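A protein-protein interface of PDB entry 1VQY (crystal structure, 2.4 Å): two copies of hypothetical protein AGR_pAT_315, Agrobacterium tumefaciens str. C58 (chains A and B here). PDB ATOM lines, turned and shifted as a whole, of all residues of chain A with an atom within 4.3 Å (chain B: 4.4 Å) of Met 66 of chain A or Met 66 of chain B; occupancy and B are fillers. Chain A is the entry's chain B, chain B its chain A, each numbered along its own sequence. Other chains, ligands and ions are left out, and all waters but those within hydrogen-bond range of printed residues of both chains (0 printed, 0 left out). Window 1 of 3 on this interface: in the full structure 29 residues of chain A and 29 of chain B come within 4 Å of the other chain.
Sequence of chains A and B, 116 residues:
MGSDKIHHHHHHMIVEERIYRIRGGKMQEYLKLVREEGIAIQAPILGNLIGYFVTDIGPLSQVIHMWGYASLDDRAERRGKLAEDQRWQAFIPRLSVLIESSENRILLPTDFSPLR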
ATOM      1  N   VAL A  15      23.363  13.991  29.083  1.00  0.00           N
ATOM      2  CA  VAL A  15      23.774  13.918  27.688  1.00  0.00           C
ATOM      3  C   VAL A  15      24.406  12.544  27.393  1.00  0.00           C
ATOM      4  O   VAL A  15      25.322  12.115  28.081  1.00  0.00           O
ATOM      5  CB  VAL A  15      24.783  15.052  27.365  1.00  0.00           C
ATOM      6  CG1 VAL A  15      25.468  14.829  26.011  1.00  0.00           C
ATOM      7  CG2 VAL A  15      24.080  16.406  27.400  1.00  0.00           C
ATOM      8  N   GLU A  16      23.914  11.863  26.366  1.00  0.00           N
ATOM      9  CA  GLU A  16      24.526  10.624  25.932  1.00  0.00           C
ATOM     10  C   GLU A  16      25.412  10.862  24.717  1.00  0.00           C
ATOM     11  O   GLU A  16      24.972  11.421  23.720  1.00  0.00           O
ATOM     12  CB  GLU A  16      23.482   9.574  25.585  1.00  0.00           C
ATOM     13  CG  GLU A  16      24.100   8.339  24.903  1.00  0.00           C
ATOM     14  CD  GLU A  16      23.094   7.270  24.555  1.00  0.00           C
ATOM     15  OE1 GLU A  16      21.896   7.582  24.384  1.00  0.00           O
ATOM     16  OE2 GLU A  16      23.514   6.109  24.468  1.00  0.00           O
ATOM     17  N   GLU A  17      26.657  10.403  24.815  1.00  0.00           N
ATOM     18  CA  GLU A  17      27.603  10.407  23.694  1.00  0.00           C
ATOM     19  C   GLU A  17      27.743   8.997  23.130  1.00  0.00           C
ATOM     20  O   GLU A  17      28.123   8.101  23.846  1.00  0.00           O
ATOM     21  CB  GLU A  17      28.970  10.921  24.155  1.00  0.00           C
ATOM     22  CG  GLU A  17      29.967  11.163  23.029  1.00  0.00           C
ATOM     23  CD  GLU A  17      31.207  11.927  23.513  1.00  0.00           C
ATOM     24  OE1 GLU A  17      31.444  11.941  24.737  1.00  0.00           O
ATOM     25  OE2 GLU A  17      31.929  12.523  22.676  1.00  0.00           O
ATOM     26  N   ASN A  48      15.795  15.072  21.652  1.00  0.00           N
ATOM     27  CA  ASN A  48      16.779  16.152  21.739  1.00  0.00           C
ATOM     28  C   ASN A  48      18.182  15.807  21.198  1.00  0.00           C
ATOM     29  O   ASN A  48      19.120  15.576  21.957  1.00  0.00           O
ATOM     30  CB  ASN A  48      16.855  16.665  23.191  1.00  0.00           C
ATOM     31  CG  ASN A  48      17.602  17.975  23.313  1.00  0.00           C
ATOM     32  OD1 ASN A  48      17.849  18.644  22.327  1.00  0.00           O
ATOM     33  ND2 ASN A  48      17.964  18.343  24.537  1.00  0.00           N
ATOM     34  N   LEU A  49      18.313  15.799  19.873  1.00  0.00           N
ATOM     35  CA  LEU A  49      19.610  15.653  19.224  1.00  0.00           C
ATOM     36  C   LEU A  49      20.413  16.920  19.470  1.00  0.00           C
ATOM     37  O   LEU A  49      19.902  18.028  19.297  1.00  0.00           O
ATOM     38  CB  LEU A  49      19.452  15.419  17.719  1.00  0.00           C
ATOM     39  CG  LEU A  49      20.735  15.382  16.890  1.00  0.00           C
ATOM     40  CD1 LEU A  49      21.628  14.257  17.300  1.00  0.00           C
ATOM     41  CD2 LEU A  49      20.413  15.248  15.419  1.00  0.00           C
ATOM     42  N   ILE A  50      21.668  16.751  19.870  1.00  0.00           N
ATOM     43  CA  ILE A  50      22.534  17.884  20.197  1.00  0.00           C
ATOM     44  C   ILE A  50      23.501  18.170  19.057  1.00  0.00           C
ATOM     45  O   ILE A  50      23.630  19.302  18.623  1.00  0.00           O
ATOM     46  CB  ILE A  50      23.365  17.615  21.481  1.00  0.00           C
ATOM     47  CG1 ILE A  50      22.457  17.252  22.664  1.00  0.00           C
ATOM     48  CG2 ILE A  50      24.278  18.802  21.794  1.00  0.00           C
ATOM     49  CD1 ILE A  50      21.812  18.411  23.304  1.00  0.00           C
ATOM     50  N   GLY A  51      24.196  17.140  18.603  1.00  0.00           N
ATOM     51  CA  GLY A  51      25.205  17.276  17.556  1.00  0.00           C
ATOM     52  C   GLY A  51      25.493  15.959  16.885  1.00  0.00           C
ATOM     53  O   GLY A  51      25.222  14.912  17.433  1.00  0.00           O
ATOM     54  N   PHE A  53      28.666  14.328  14.336  1.00  0.00           N
ATOM     55  CA  PHE A  53      29.995  14.698  13.860  1.00  0.00           C
ATOM     56  C   PHE A  53      30.730  13.544  13.179  1.00  0.00           C
ATOM     57  O   PHE A  53      30.489  12.382  13.468  1.00  0.00           O
ATOM     58  CB  PHE A  53      30.870  15.189  15.015  1.00  0.00           C
ATOM     59  CG  PHE A  53      30.217  16.203  15.911  1.00  0.00           C
ATOM     60  CD1 PHE A  53      30.121  17.539  15.526  1.00  0.00           C
ATOM     61  CD2 PHE A  53      29.736  15.833  17.164  1.00  0.00           C
ATOM     62  CE1 PHE A  53      29.533  18.476  16.347  1.00  0.00           C
ATOM     63  CE2 PHE A  53      29.148  16.773  18.008  1.00  0.00           C
ATOM     64  CZ  PHE A  53      29.042  18.100  17.592  1.00  0.00           C
ATOM     65  N   HIS A  65      27.738  11.192  17.977  1.00  0.00           N
ATOM     66  CA  HIS A  65      26.473  11.932  18.136  1.00  0.00           C
ATOM     67  C   HIS A  65      26.027  12.052  19.589  1.00  0.00           C
ATOM     68  O   HIS A  65      26.219  11.139  20.395  1.00  0.00           O
ATOM     69  CB  HIS A  65      25.340  11.390  17.253  1.00  0.00           C
ATOM     70  CG  HIS A  65      25.285   9.896  17.140  1.00  0.00           C
ATOM     71  ND1 HIS A  65      24.208   9.158  17.577  1.00  0.00           N
ATOM     72  CD2 HIS A  65      26.141   9.010  16.579  1.00  0.00           C
ATOM     73  CE1 HIS A  65      24.410   7.881  17.317  1.00  0.00           C
ATOM     74  NE2 HIS A  65      25.581   7.764  16.716  1.00  0.00           N
ATOM     75  N   MET A  66      25.457  13.212  19.909  1.00  0.00           N
ATOM     76  CA  MET A  66      25.034  13.531  21.262  1.00  0.00           C
ATOM     77  C   MET A  66      23.543  13.745  21.370  1.00  0.00           C
ATOM     78  O   MET A  66      22.931  14.403  20.521  1.00  0.00           O
ATOM     79  CB  MET A  66      25.759  14.766  21.769  1.00  0.00           C
ATOM     80  CG  MET A  66      27.050  14.451  22.502  1.00  0.00           C
ATOM     81  SD  MET A  66      28.159  16.070  22.560  1.00  0.00           S
ATOM     82  CE  MET A  66      29.481  15.459  23.747  1.00  0.00           C
ATOM     83  N   TRP A  67      22.979  13.201  22.447  1.00  0.00           N
ATOM     84  CA  TRP A  67      21.537  13.210  22.686  1.00  0.00           C
ATOM     85  C   TRP A  67      21.235  13.692  24.082  1.00  0.00           C
ATOM     86  O   TRP A  67      21.823  13.181  25.038  1.00  0.00           O
ATOM     87  CB  TRP A  67      20.976  11.810  22.522  1.00  0.00           C
ATOM     88  CG  TRP A  67      21.162  11.273  21.127  1.00  0.00           C
ATOM     89  CD1 TRP A  67      22.214  10.554  20.672  1.00  0.00           C
ATOM     90  CD2 TRP A  67      20.276  11.443  20.006  1.00  0.00           C
ATOM     91  NE1 TRP A  67      22.041  10.246  19.344  1.00  0.00           N
ATOM     92  CE2 TRP A  67      20.862  10.781  18.908  1.00  0.00           C
ATOM     93  CE3 TRP A  67      19.048  12.090  19.826  1.00  0.00           C
ATOM     94  CZ2 TRP A  67      20.249  10.718  17.649  1.00  0.00           C
ATOM     95  CZ3 TRP A  67      18.450  12.055  18.579  1.00  0.00           C
ATOM     96  CH2 TRP A  67      19.046  11.370  17.501  1.00  0.00           C
ATOM     97  N   LEU A 107      27.135  11.698  30.137  1.00  0.00           N
ATOM     98  CA  LEU A 107      27.800  12.909  30.568  1.00  0.00           C
ATOM     99  C   LEU A 107      26.841  13.821  31.352  1.00  0.00           C
ATOM    100  O   LEU A 107      25.691  14.047  30.957  1.00  0.00           O
ATOM    101  CB  LEU A 107      28.326  13.643  29.344  1.00  0.00           C
ATOM    102  CG  LEU A 107      29.080  12.822  28.292  1.00  0.00           C
ATOM    103  CD1 LEU A 107      29.507  13.685  27.120  1.00  0.00           C
ATOM    104  CD2 LEU A 107      30.282  12.159  28.895  1.00  0.00           C
ATOM    105  N   VAL B  15      34.363  21.858  15.410  1.00  0.00           N
ATOM    106  CA  VAL B  15      34.256  21.552  16.822  1.00  0.00           C
ATOM    107  C   VAL B  15      35.497  20.811  17.340  1.00  0.00           C
ATOM    108  O   VAL B  15      35.907  19.813  16.787  1.00  0.00           O
ATOM    109  CB  VAL B  15      32.975  20.738  17.068  1.00  0.00           C
ATOM    110  CG1 VAL B  15      32.911  20.218  18.489  1.00  0.00           C
ATOM    111  CG2 VAL B  15      31.759  21.602  16.740  1.00  0.00           C
ATOM    112  N   GLU B  16      36.108  21.341  18.391  1.00  0.00           N
ATOM    113  CA  GLU B  16      37.169  20.644  19.113  1.00  0.00           C
ATOM    114  C   GLU B  16      36.575  19.977  20.349  1.00  0.00           C
ATOM    115  O   GLU B  16      35.897  20.618  21.151  1.00  0.00           O
ATOM    116  CB  GLU B  16      38.288  21.612  19.533  1.00  0.00           C
ATOM    117  CG  GLU B  16      39.545  20.910  20.075  1.00  0.00           C
ATOM    118  CD  GLU B  16      40.606  21.857  20.618  1.00  0.00           C
ATOM    119  OE1 GLU B  16      40.575  23.088  20.373  1.00  0.00           O
ATOM    120  OE2 GLU B  16      41.511  21.354  21.295  1.00  0.00           O
ATOM    121  N   GLU B  17      36.808  18.676  20.484  1.00  0.00           N
ATOM    122  CA  GLU B  17      36.456  17.955  21.698  1.00  0.00           C
ATOM    123  C   GLU B  17      37.752  17.652  22.424  1.00  0.00           C
ATOM    124  O   GLU B  17      38.672  17.066  21.847  1.00  0.00           O
ATOM    125  CB  GLU B  17      35.720  16.649  21.393  1.00  0.00           C
ATOM    126  CG  GLU B  17      35.268  15.892  22.666  1.00  0.00           C
ATOM    127  CD  GLU B  17      34.436  14.678  22.339  1.00  0.00           C
ATOM    128  OE1 GLU B  17      34.532  14.217  21.202  1.00  0.00           O
ATOM    129  OE2 GLU B  17      33.686  14.179  23.207  1.00  0.00           O
ATOM    130  N   ASN B  48      33.649  30.329  21.947  1.00  0.00           N
ATOM    131  CA  ASN B  48      32.425  29.551  21.870  1.00  0.00           C
ATOM    132  C   ASN B  48      32.501  28.209  22.592  1.00  0.00           C
ATOM    133  O   ASN B  48      32.550  27.139  21.955  1.00  0.00           O
ATOM    134  CB  ASN B  48      32.031  29.356  20.403  1.00  0.00           C
ATOM    135  CG  ASN B  48      30.766  28.536  20.248  1.00  0.00           C
ATOM    136  OD1 ASN B  48      30.058  28.293  21.221  1.00  0.00           O
ATOM    137  ND2 ASN B  48      30.481  28.104  19.028  1.00  0.00           N
ATOM    138  N   LEU B  49      32.496  28.267  23.924  1.00  0.00           N
ATOM    139  CA  LEU B  49      32.277  27.069  24.745  1.00  0.00           C
ATOM    140  C   LEU B  49      30.898  26.517  24.414  1.00  0.00           C
ATOM    141  O   LEU B  49      29.898  27.215  24.561  1.00  0.00           O
ATOM    142  CB  LEU B  49      32.352  27.401  26.236  1.00  0.00           C
ATOM    143  CG  LEU B  49      32.225  26.224  27.225  1.00  0.00           C
ATOM    144  CD1 LEU B  49      33.245  25.150  26.955  1.00  0.00           C
ATOM    145  CD2 LEU B  49      32.337  26.696  28.675  1.00  0.00           C
ATOM    146  N   ILE B  50      30.844  25.278  23.947  1.00  0.00           N
ATOM    147  CA  ILE B  50      29.580  24.659  23.592  1.00  0.00           C
ATOM    148  C   ILE B  50      29.044  23.893  24.793  1.00  0.00           C
ATOM    149  O   ILE B  50      27.882  24.027  25.152  1.00  0.00           O
ATOM    150  CB  ILE B  50      29.759  23.719  22.385  1.00  0.00           C
ATOM    151  CG1 ILE B  50      30.139  24.543  21.148  1.00  0.00           C
ATOM    152  CG2 ILE B  50      28.508  22.849  22.152  1.00  0.00           C
ATOM    153  CD1 ILE B  50      30.386  23.734  19.944  1.00  0.00           C
ATOM    154  N   GLY B  51      29.903  23.090  25.407  1.00  0.00           N
ATOM    155  CA  GLY B  51      29.521  22.292  26.575  1.00  0.00           C
ATOM    156  C   GLY B  51      30.697  21.823  27.413  1.00  0.00           C
ATOM    157  O   GLY B  51      31.830  21.824  26.943  1.00  0.00           O
ATOM    158  N   PHE B  53      31.437  18.764  30.548  1.00  0.00           N
ATOM    159  CA  PHE B  53      30.794  17.581  31.144  1.00  0.00           C
ATOM    160  C   PHE B  53      31.729  16.717  31.987  1.00  0.00           C
ATOM    161  O   PHE B  53      32.936  16.654  31.737  1.00  0.00           O
ATOM    162  CB  PHE B  53      30.204  16.681  30.055  1.00  0.00           C
ATOM    163  CG  PHE B  53      29.430  17.415  28.965  1.00  0.00           C
ATOM    164  CD1 PHE B  53      28.072  17.632  29.079  1.00  0.00           C
ATOM    165  CD2 PHE B  53      30.071  17.841  27.805  1.00  0.00           C
ATOM    166  CE1 PHE B  53      27.364  18.267  28.062  1.00  0.00           C
ATOM    167  CE2 PHE B  53      29.369  18.467  26.767  1.00  0.00           C
ATOM    168  CZ  PHE B  53      28.016  18.682  26.896  1.00  0.00           C
ATOM    169  N   HIS B  65      35.190  18.674  27.319  1.00  0.00           N
ATOM    170  CA  HIS B  65      34.730  19.991  26.875  1.00  0.00           C
ATOM    171  C   HIS B  65      34.794  20.183  25.358  1.00  0.00           C
ATOM    172  O   HIS B  65      35.691  19.705  24.682  1.00  0.00           O
ATOM    173  CB  HIS B  65      35.371  21.170  27.638  1.00  0.00           C
ATOM    174  CG  HIS B  65      36.816  21.003  27.999  1.00  0.00           C
ATOM    175  ND1 HIS B  65      37.771  21.944  27.668  1.00  0.00           N
ATOM    176  CD2 HIS B  65      37.456  20.068  28.741  1.00  0.00           C
ATOM    177  CE1 HIS B  65      38.943  21.570  28.149  1.00  0.00           C
ATOM    178  NE2 HIS B  65      38.778  20.438  28.809  1.00  0.00           N
ATOM    179  N   MET B  66      33.784  20.873  24.840  1.00  0.00           N
ATOM    180  CA  MET B  66      33.674  21.153  23.435  1.00  0.00           C
ATOM    181  C   MET B  66      33.690  22.632  23.202  1.00  0.00           C
ATOM    182  O   MET B  66      33.067  23.405  23.936  1.00  0.00           O
ATOM    183  CB  MET B  66      32.410  20.578  22.854  1.00  0.00           C
ATOM    184  CG  MET B  66      32.571  19.154  22.294  1.00  0.00           C
ATOM    185  SD  MET B  66      30.822  18.293  22.087  1.00  0.00           S
ATOM    186  CE  MET B  66      30.078  19.474  20.852  1.00  0.00           C
ATOM    187  N   TRP B  67      34.410  22.986  22.143  1.00  0.00           N
ATOM    188  CA  TRP B  67      34.636  24.355  21.726  1.00  0.00           C
ATOM    189  C   TRP B  67      34.331  24.440  20.237  1.00  0.00           C
ATOM    190  O   TRP B  67      34.649  23.527  19.459  1.00  0.00           O
ATOM    191  CB  TRP B  67      36.091  24.719  21.977  1.00  0.00           C
ATOM    192  CG  TRP B  67      36.469  24.626  23.410  1.00  0.00           C
ATOM    193  CD1 TRP B  67      36.972  23.541  24.059  1.00  0.00           C
ATOM    194  CD2 TRP B  67      36.362  25.669  24.383  1.00  0.00           C
ATOM    195  NE1 TRP B  67      37.191  23.843  25.381  1.00  0.00           N
ATOM    196  CE2 TRP B  67      36.821  25.145  25.606  1.00  0.00           C
ATOM    197  CE3 TRP B  67      35.922  27.003  24.336  1.00  0.00           C
ATOM    198  CZ2 TRP B  67      36.865  25.901  26.766  1.00  0.00           C
ATOM    199  CZ3 TRP B  67      35.964  27.764  25.502  1.00  0.00           C
ATOM    200  CH2 TRP B  67      36.424  27.208  26.697  1.00  0.00           C
ATOM    201  N   LEU B 115      24.246  21.354  15.852  1.00  0.00           N
ATOM    202  CA  LEU B 115      25.428  22.170  16.010  1.00  0.00           C
ATOM    203  C   LEU B 115      26.182  22.094  14.725  1.00  0.00           C
ATOM    204  O   LEU B 115      26.791  21.068  14.450  1.00  0.00           O
ATOM    205  CB  LEU B 115      26.322  21.636  17.134  1.00  0.00           C
ATOM    206  CG  LEU B 115      25.999  22.103  18.549  1.00  0.00           C
ATOM    207  CD1 LEU B 115      26.955  21.442  19.495  1.00  0.00           C
ATOM    208  CD2 LEU B 115      26.117  23.581  18.676  1.00  0.00           C
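Hydrophobic or aromatic side chains of chain B within 4 Å of the printed part of chain A: Val 15, Phe 53, Met 66 and Leu 115. Of the 12 printed residues of chain A, 6 touch a printed residue of chain B.
Val 15 of chain A touches Phe 53 of chain B, and with the chains exchanged Phe 53 of chain A touches Val 15 of chain B. Glu 17 of chain B touches its own counterpart, Glu 17 of chain A. Phe 53 of chain A touches Met 66 of chain B, but with the chains exchanged Met 66 of chain A does not touch Phe 53 of chain B (4.3 Å). Met 66 of chain B touches its own counterpart, Met 66 of chain A. Of the 7 pairs that touch across the chains among the printed residues, 4 have their exchanged pair printed and touching as well.
The side-chain sulfur (SD) of Met 66 of chain B sits close to the side-chain sulfur (SD) of Met 66 of chain A. The side-chain carboxylate (OE2) of Glu 17 of chain A lies close to the side-chain carboxylate (OE2) of Glu 17 of chain B.
The backbone carbonyl oxygen (O) of Gly 51 of chain A lies within hydrogen-bond range of the backbone NH (N) of Met 66 of chain A, 3.0 Å away. The backbone carbonyl oxygen (O) of Gly 51 of chain B is in hydrogen-bond range of the backbone NH (N) of Met 66 of chain B, 3.0 Å away. The backbone NH (N) of Leu 107 of chain A lies within hydrogen-bond range of the backbone carbonyl oxygen (O) of Val 15 of chain A, at 2.8 Å. The backbone carbonyl oxygen (O) of Met 66 of chain B is in hydrogen-bond range of the backbone NH (N) of Ile 50 of chain B (2.9 Å). The backbone carbonyl oxygen (O) of Met 66 of chain A lies within hydrogen-bond range of the backbone NH (N) of Ile 50 of chain A, at 2.7 Å.
Glu 16 of chain A touches none of the printed residues of chain B. Printed residues of chain B within 4 Å of Glu 17 of chain A: Glu 17. Printed residues of chain B within 4 Å of Ile 50 of chain A: Leu 115 (3.5 Å). Printed residues of chain B within 4 Å of Phe 53 of chain A: Val 15 (3.9 Å) and Met 66 (3.7 Å). Met 66 of chain A touches just one residue of chain B: Met 66 (3.5 Å). Of the printed residues of chain A, Phe 53 of chain B touches Val 15 and Leu 107. Of chain A, only Phe 53 and Met 66 come within 4 Å of Met 66 of chain B.
Among the printed residues, merely in contact across the chains: Val 15 of chain A with Phe 53 of chain B (3.8 Å), Ile 50 of chain A with Leu 115 of chain B (3.5 Å), Phe 53 of chain A with Val 15 of chain B (3.9 Å), Phe 53 of chain A with Met 66 of chain B (3.7 Å) and Leu 107 of chain A with Phe 53 of chain B (3.6 Å).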
